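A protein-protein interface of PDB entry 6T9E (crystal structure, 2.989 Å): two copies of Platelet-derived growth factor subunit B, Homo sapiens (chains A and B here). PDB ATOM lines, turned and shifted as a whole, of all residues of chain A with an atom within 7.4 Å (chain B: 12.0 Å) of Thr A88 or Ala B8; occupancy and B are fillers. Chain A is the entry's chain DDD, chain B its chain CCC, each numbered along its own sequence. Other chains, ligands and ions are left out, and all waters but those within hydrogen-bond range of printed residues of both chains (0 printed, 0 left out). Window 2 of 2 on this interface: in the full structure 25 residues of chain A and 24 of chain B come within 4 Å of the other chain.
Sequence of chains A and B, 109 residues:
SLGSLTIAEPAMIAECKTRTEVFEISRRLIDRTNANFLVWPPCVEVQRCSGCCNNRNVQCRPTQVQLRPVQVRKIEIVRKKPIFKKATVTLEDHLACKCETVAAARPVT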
ATOM      1  N   LEU A  29       7.248   6.765  -5.949  1.00  0.00           N
ATOM      2  CA  LEU A  29       5.982   7.486  -5.947  1.00  0.00           C
ATOM      3  C   LEU A  29       6.004   8.684  -4.997  1.00  0.00           C
ATOM      4  O   LEU A  29       5.182   9.581  -5.161  1.00  0.00           O
ATOM      5  CB  LEU A  29       4.814   6.534  -5.656  1.00  0.00           C
ATOM      6  CG  LEU A  29       4.078   6.022  -6.898  1.00  0.00           C
ATOM      7  CD1 LEU A  29       4.826   4.862  -7.551  1.00  0.00           C
ATOM      8  CD2 LEU A  29       2.643   5.626  -6.578  1.00  0.00           C
ATOM      9  N   ILE A  30       6.937   8.708  -4.022  1.00  0.00           N
ATOM     10  CA  ILE A  30       7.092   9.840  -3.106  1.00  0.00           C
ATOM     11  C   ILE A  30       8.482  10.493  -3.193  1.00  0.00           C
ATOM     12  O   ILE A  30       8.601  11.699  -2.970  1.00  0.00           O
ATOM     13  CB  ILE A  30       6.720   9.483  -1.650  1.00  0.00           C
ATOM     14  CG1 ILE A  30       5.354   8.800  -1.561  1.00  0.00           C
ATOM     15  CG2 ILE A  30       6.781  10.719  -0.761  1.00  0.00           C
ATOM     16  CD1 ILE A  30       5.043   8.214  -0.206  1.00  0.00           C
ATOM     17  N   ARG A  68      -8.628   8.732  -6.961  1.00  0.00           N
ATOM     18  CA  ARG A  68      -8.880   8.650  -5.530  1.00  0.00           C
ATOM     19  C   ARG A  68      -7.575   8.940  -4.794  1.00  0.00           C
ATOM     20  O   ARG A  68      -6.694   8.084  -4.735  1.00  0.00           O
ATOM     21  CB  ARG A  68      -9.417   7.274  -5.129  1.00  0.00           C
ATOM     22  CG  ARG A  68      -9.567   7.113  -3.626  1.00  0.00           C
ATOM     23  CD  ARG A  68     -10.056   5.737  -3.224  1.00  0.00           C
ATOM     24  NE  ARG A  68      -9.425   4.634  -3.935  1.00  0.00           N
ATOM     25  CZ  ARG A  68      -9.299   3.394  -3.460  1.00  0.00           C
ATOM     26  NH1 ARG A  68      -9.727   3.095  -2.245  1.00  0.00           N
ATOM     27  NH2 ARG A  68      -8.733   2.456  -4.198  1.00  0.00           N
ATOM     28  N   PRO A  69      -7.410  10.163  -4.232  1.00  0.00           N
ATOM     29  CA  PRO A  69      -6.234  10.486  -3.422  1.00  0.00           C
ATOM     30  C   PRO A  69      -6.379   9.949  -1.999  1.00  0.00           C
ATOM     31  O   PRO A  69      -7.478   9.899  -1.437  1.00  0.00           O
ATOM     32  CB  PRO A  69      -6.201  12.022  -3.467  1.00  0.00           C
ATOM     33  CG  PRO A  69      -7.656  12.451  -3.658  1.00  0.00           C
ATOM     34  CD  PRO A  69      -8.351  11.294  -4.342  1.00  0.00           C
ATOM     35  N   VAL A  70      -5.255   9.516  -1.433  1.00  0.00           N
ATOM     36  CA  VAL A  70      -5.315   8.889  -0.128  1.00  0.00           C
ATOM     37  C   VAL A  70      -4.097   9.350   0.643  1.00  0.00           C
ATOM     38  O   VAL A  70      -3.029   9.470   0.040  1.00  0.00           O
ATOM     39  CB  VAL A  70      -5.285   7.355  -0.233  1.00  0.00           C
ATOM     40  CG1 VAL A  70      -6.628   6.767  -0.647  1.00  0.00           C
ATOM     41  CG2 VAL A  70      -4.150   6.889  -1.135  1.00  0.00           C
ATOM     42  N   GLN A  71      -4.282   9.536   1.960  1.00  0.00           N
ATOM     43  CA  GLN A  71      -3.199   9.952   2.834  1.00  0.00           C
ATOM     44  C   GLN A  71      -2.550   8.724   3.459  1.00  0.00           C
ATOM     45  O   GLN A  71      -3.245   7.796   3.880  1.00  0.00           O
ATOM     46  CB  GLN A  71      -3.669  10.948   3.892  1.00  0.00           C
ATOM     47  CG  GLN A  71      -2.523  11.642   4.622  1.00  0.00           C
ATOM     48  CD  GLN A  71      -2.913  12.990   5.183  1.00  0.00           C
ATOM     49  OE1 GLN A  71      -3.551  13.097   6.235  1.00  0.00           O
ATOM     50  NE2 GLN A  71      -2.498  14.045   4.496  1.00  0.00           N
ATOM     51  N   VAL A  72      -1.210   8.754   3.459  1.00  0.00           N
ATOM     52  CA  VAL A  72      -0.344   7.763   4.077  1.00  0.00           C
ATOM     53  C   VAL A  72       0.665   8.488   4.966  1.00  0.00           C
ATOM     54  O   VAL A  72       0.569   9.696   5.131  1.00  0.00           O
ATOM     55  CB  VAL A  72       0.351   6.896   3.014  1.00  0.00           C
ATOM     56  CG1 VAL A  72      -0.656   6.255   2.075  1.00  0.00           C
ATOM     57  CG2 VAL A  72       1.434   7.650   2.256  1.00  0.00           C
ATOM     58  N   ARG A  73       1.609   7.752   5.557  1.00  0.00           N
ATOM     59  CA  ARG A  73       2.693   8.368   6.302  1.00  0.00           C
ATOM     60  C   ARG A  73       4.045   7.977   5.708  1.00  0.00           C
ATOM     61  O   ARG A  73       4.284   6.821   5.382  1.00  0.00           O
ATOM     62  CB  ARG A  73       2.614   7.955   7.769  1.00  0.00           C
ATOM     63  CG  ARG A  73       1.451   8.580   8.527  1.00  0.00           C
ATOM     64  CD  ARG A  73       1.816   9.830   9.330  1.00  0.00           C
ATOM     65  NE  ARG A  73       1.036  10.145  10.536  1.00  0.00           N
ATOM     66  CZ  ARG A  73      -0.245   9.809  10.799  1.00  0.00           C
ATOM     67  NH1 ARG A  73      -1.002   9.130   9.947  1.00  0.00           N
ATOM     68  NH2 ARG A  73      -0.782  10.182  11.943  1.00  0.00           N
ATOM     69  N   LYS A  86       3.044  13.241   6.948  1.00  0.00           N
ATOM     70  CA  LYS A  86       1.904  12.791   6.157  1.00  0.00           C
ATOM     71  C   LYS A  86       2.222  12.981   4.669  1.00  0.00           C
ATOM     72  O   LYS A  86       3.050  13.821   4.315  1.00  0.00           O
ATOM     73  CB  LYS A  86       0.611  13.455   6.626  1.00  0.00           C
ATOM     74  CG  LYS A  86       0.320  13.216   8.090  1.00  0.00           C
ATOM     75  CD  LYS A  86      -0.960  13.836   8.539  1.00  0.00           C
ATOM     76  CE  LYS A  86      -1.120  13.751  10.039  1.00  0.00           C
ATOM     77  NZ  LYS A  86      -2.507  13.385  10.405  1.00  0.00           N
ATOM     78  N   ALA A  87       1.626  12.141   3.804  1.00  0.00           N
ATOM     79  CA  ALA A  87       1.808  12.222   2.356  1.00  0.00           C
ATOM     80  C   ALA A  87       0.568  11.677   1.657  1.00  0.00           C
ATOM     81  O   ALA A  87      -0.061  10.726   2.122  1.00  0.00           O
ATOM     82  CB  ALA A  87       3.060  11.510   1.887  1.00  0.00           C
ATOM     83  N   THR A  88       0.211  12.323   0.545  1.00  0.00           N
ATOM     84  CA  THR A  88      -0.951  11.909  -0.223  1.00  0.00           C
ATOM     85  C   THR A  88      -0.469  11.171  -1.465  1.00  0.00           C
ATOM     86  O   THR A  88       0.514  11.588  -2.077  1.00  0.00           O
ATOM     87  CB  THR A  88      -1.909  13.078  -0.508  1.00  0.00           C
ATOM     88  OG1 THR A  88      -2.633  13.373   0.689  1.00  0.00           O
ATOM     89  CG2 THR A  88      -2.924  12.772  -1.590  1.00  0.00           C
ATOM     90  N   VAL A  89      -1.149  10.066  -1.791  1.00  0.00           N
ATOM     91  CA  VAL A  89      -0.944   9.439  -3.083  1.00  0.00           C
ATOM     92  C   VAL A  89      -2.297   9.276  -3.755  1.00  0.00           C
ATOM     93  O   VAL A  89      -3.317   9.161  -3.071  1.00  0.00           O
ATOM     94  CB  VAL A  89      -0.163   8.117  -3.029  1.00  0.00           C
ATOM     95  CG1 VAL A  89       1.321   8.319  -2.753  1.00  0.00           C
ATOM     96  CG2 VAL A  89      -0.805   7.087  -2.109  1.00  0.00           C
ATOM     97  N   THR A  90      -2.262   9.341  -5.092  1.00  0.00           N
ATOM     98  CA  THR A  90      -3.456   9.259  -5.902  1.00  0.00           C
ATOM     99  C   THR A  90      -3.524   7.885  -6.531  1.00  0.00           C
ATOM    100  O   THR A  90      -2.586   7.460  -7.208  1.00  0.00           O
ATOM    101  CB  THR A  90      -3.535  10.382  -6.929  1.00  0.00           C
ATOM    102  OG1 THR A  90      -4.444  11.215  -6.218  1.00  0.00           O
ATOM    103  CG2 THR A  90      -4.146   9.957  -8.247  1.00  0.00           C
ATOM    104  N   ILE B   7      -9.651  16.920  -1.546  1.00  0.00           N
ATOM    105  CA  ILE B   7      -8.920  16.804  -0.247  1.00  0.00           C
ATOM    106  C   ILE B   7      -8.910  15.344   0.176  1.00  0.00           C
ATOM    107  O   ILE B   7      -9.974  14.731   0.234  1.00  0.00           O
ATOM    108  CB  ILE B   7      -9.570  17.665   0.809  1.00  0.00           C
ATOM    109  N   ALA B   8      -7.704  14.848   0.525  1.00  0.00           N
ATOM    110  CA  ALA B   8      -7.378  13.442   0.777  1.00  0.00           C
ATOM    111  C   ALA B   8      -8.247  12.819   1.873  1.00  0.00           C
ATOM    112  O   ALA B   8      -8.933  13.533   2.613  1.00  0.00           O
ATOM    113  CB  ALA B   8      -5.903  13.266   1.087  1.00  0.00           C
ATOM    114  N   GLU B   9      -8.215  11.473   1.935  1.00  0.00           N
ATOM    115  CA  GLU B   9      -8.815  10.690   3.011  1.00  0.00           C
ATOM    116  C   GLU B   9      -7.865   9.560   3.419  1.00  0.00           C
ATOM    117  O   GLU B   9      -6.863   9.302   2.755  1.00  0.00           O
ATOM    118  CB  GLU B   9     -10.295  10.343   2.771  1.00  0.00           C
ATOM    119  CG  GLU B   9     -10.572   9.029   2.066  1.00  0.00           C
ATOM    120  CD  GLU B   9     -10.758   9.102   0.553  1.00  0.00           C
ATOM    121  OE1 GLU B   9     -10.374  10.133  -0.046  1.00  0.00           O
ATOM    122  OE2 GLU B   9     -11.274   8.111  -0.031  1.00  0.00           O
ATOM    123  N   PRO B  10      -8.113   8.869   4.554  1.00  0.00           N
ATOM    124  CA  PRO B  10      -7.072   8.061   5.186  1.00  0.00           C
ATOM    125  C   PRO B  10      -6.966   6.647   4.614  1.00  0.00           C
ATOM    126  O   PRO B  10      -7.947   5.896   4.582  1.00  0.00           O
ATOM    127  CB  PRO B  10      -7.568   8.025   6.637  1.00  0.00           C
ATOM    128  CG  PRO B  10      -9.084   7.982   6.506  1.00  0.00           C
ATOM    129  CD  PRO B  10      -9.401   8.800   5.270  1.00  0.00           C
ATOM    130  N   ALA B  11      -5.739   6.289   4.211  1.00  0.00           N
ATOM    131  CA  ALA B  11      -5.429   5.025   3.558  1.00  0.00           C
ATOM    132  C   ALA B  11      -5.716   3.809   4.455  1.00  0.00           C
ATOM    133  O   ALA B  11      -5.381   3.799   5.640  1.00  0.00           O
ATOM    134  CB  ALA B  11      -3.991   5.056   3.096  1.00  0.00           C
ATOM    135  N   MET B  12      -6.322   2.769   3.858  1.00  0.00           N
ATOM    136  CA  MET B  12      -6.624   1.494   4.492  1.00  0.00           C
ATOM    137  C   MET B  12      -5.696   0.416   3.942  1.00  0.00           C
ATOM    138  O   MET B  12      -5.596   0.248   2.722  1.00  0.00           O
ATOM    139  CB  MET B  12      -8.043   1.066   4.125  1.00  0.00           C
ATOM    140  CG  MET B  12      -9.085   2.107   4.435  1.00  0.00           C
ATOM    141  SD  MET B  12      -9.820   1.870   6.077  1.00  0.00           S
ATOM    142  CE  MET B  12     -10.114   0.098   6.109  1.00  0.00           C
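N of Gln A71 is in hydrogen-bond range of O of Glu B9 (2.7 Å). The backbone NH (N) of Ala B11 sits at hydrogen-bond distance from the backbone carbonyl oxygen (O) of Gln A71, at 2.9 Å. OE1 of Glu B9 lies close to O of Pro A69 (3.2 Å).
N of Val A70 is in hydrogen-bond range of O of Val A89 (2.6 Å). The backbone NH (N) of Val A72 is in hydrogen-bond range of the backbone carbonyl oxygen (O) of Ala A87 (2.6 Å).
Glu B9 touches Val A70. Gln A71 touches Pro B10. Ala B11 touches Val A72. Thr A88 touches Ala B8 (OG1 to CB, 3.3 Å).
Thr A88 touches just one residue of chain B: Ala B8. Ala B8 touches one residue of chain A. Of chain B, only Glu B9 comes within 4 Å of Pro A69. Of the printed residues of chain B, Val A70 touches Glu B9. No residue of chain B comes within 4 Å of Ala A87. No residue of chain B comes within 4 Å of Val A89. No residue of chain B comes within 4 Å of Thr A90. Printed residues of chain A within 4 Å of Pro B10: Gln A71. Of the printed residues of chain A, Ala B11 touches Gln A71 (2.9 Å) and Val A72 (3.7 Å). Printed residues of chain A within 4 Å of Glu B9: Pro A69, Val A70 and Gln A71. The nearest residue of chain B that does not touch Thr A88 is Glu B9 (6.0 Å). The nearest printed residue of chain A that does not touch Ala B8 is Gln A71 (4.2 Å).
Of the 6 printed residues of chain B, 4 touch a printed residue of chain A. Along chain B the printed residues that touch a printed residue of chain A span positions 8 to 11. Of the 13 printed residues of chain A, 5 touch a printed residue of chain B. Hydrophobic or aromatic side chains of chain A within 4 Å of the printed part of chain B: Val A70 and Val A72. Among the printed residues, no Asp or Glu carboxylate lies within 4 Å of a Lys or Arg side-chain nitrogen of the other chain.
No position is printed for both chains.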
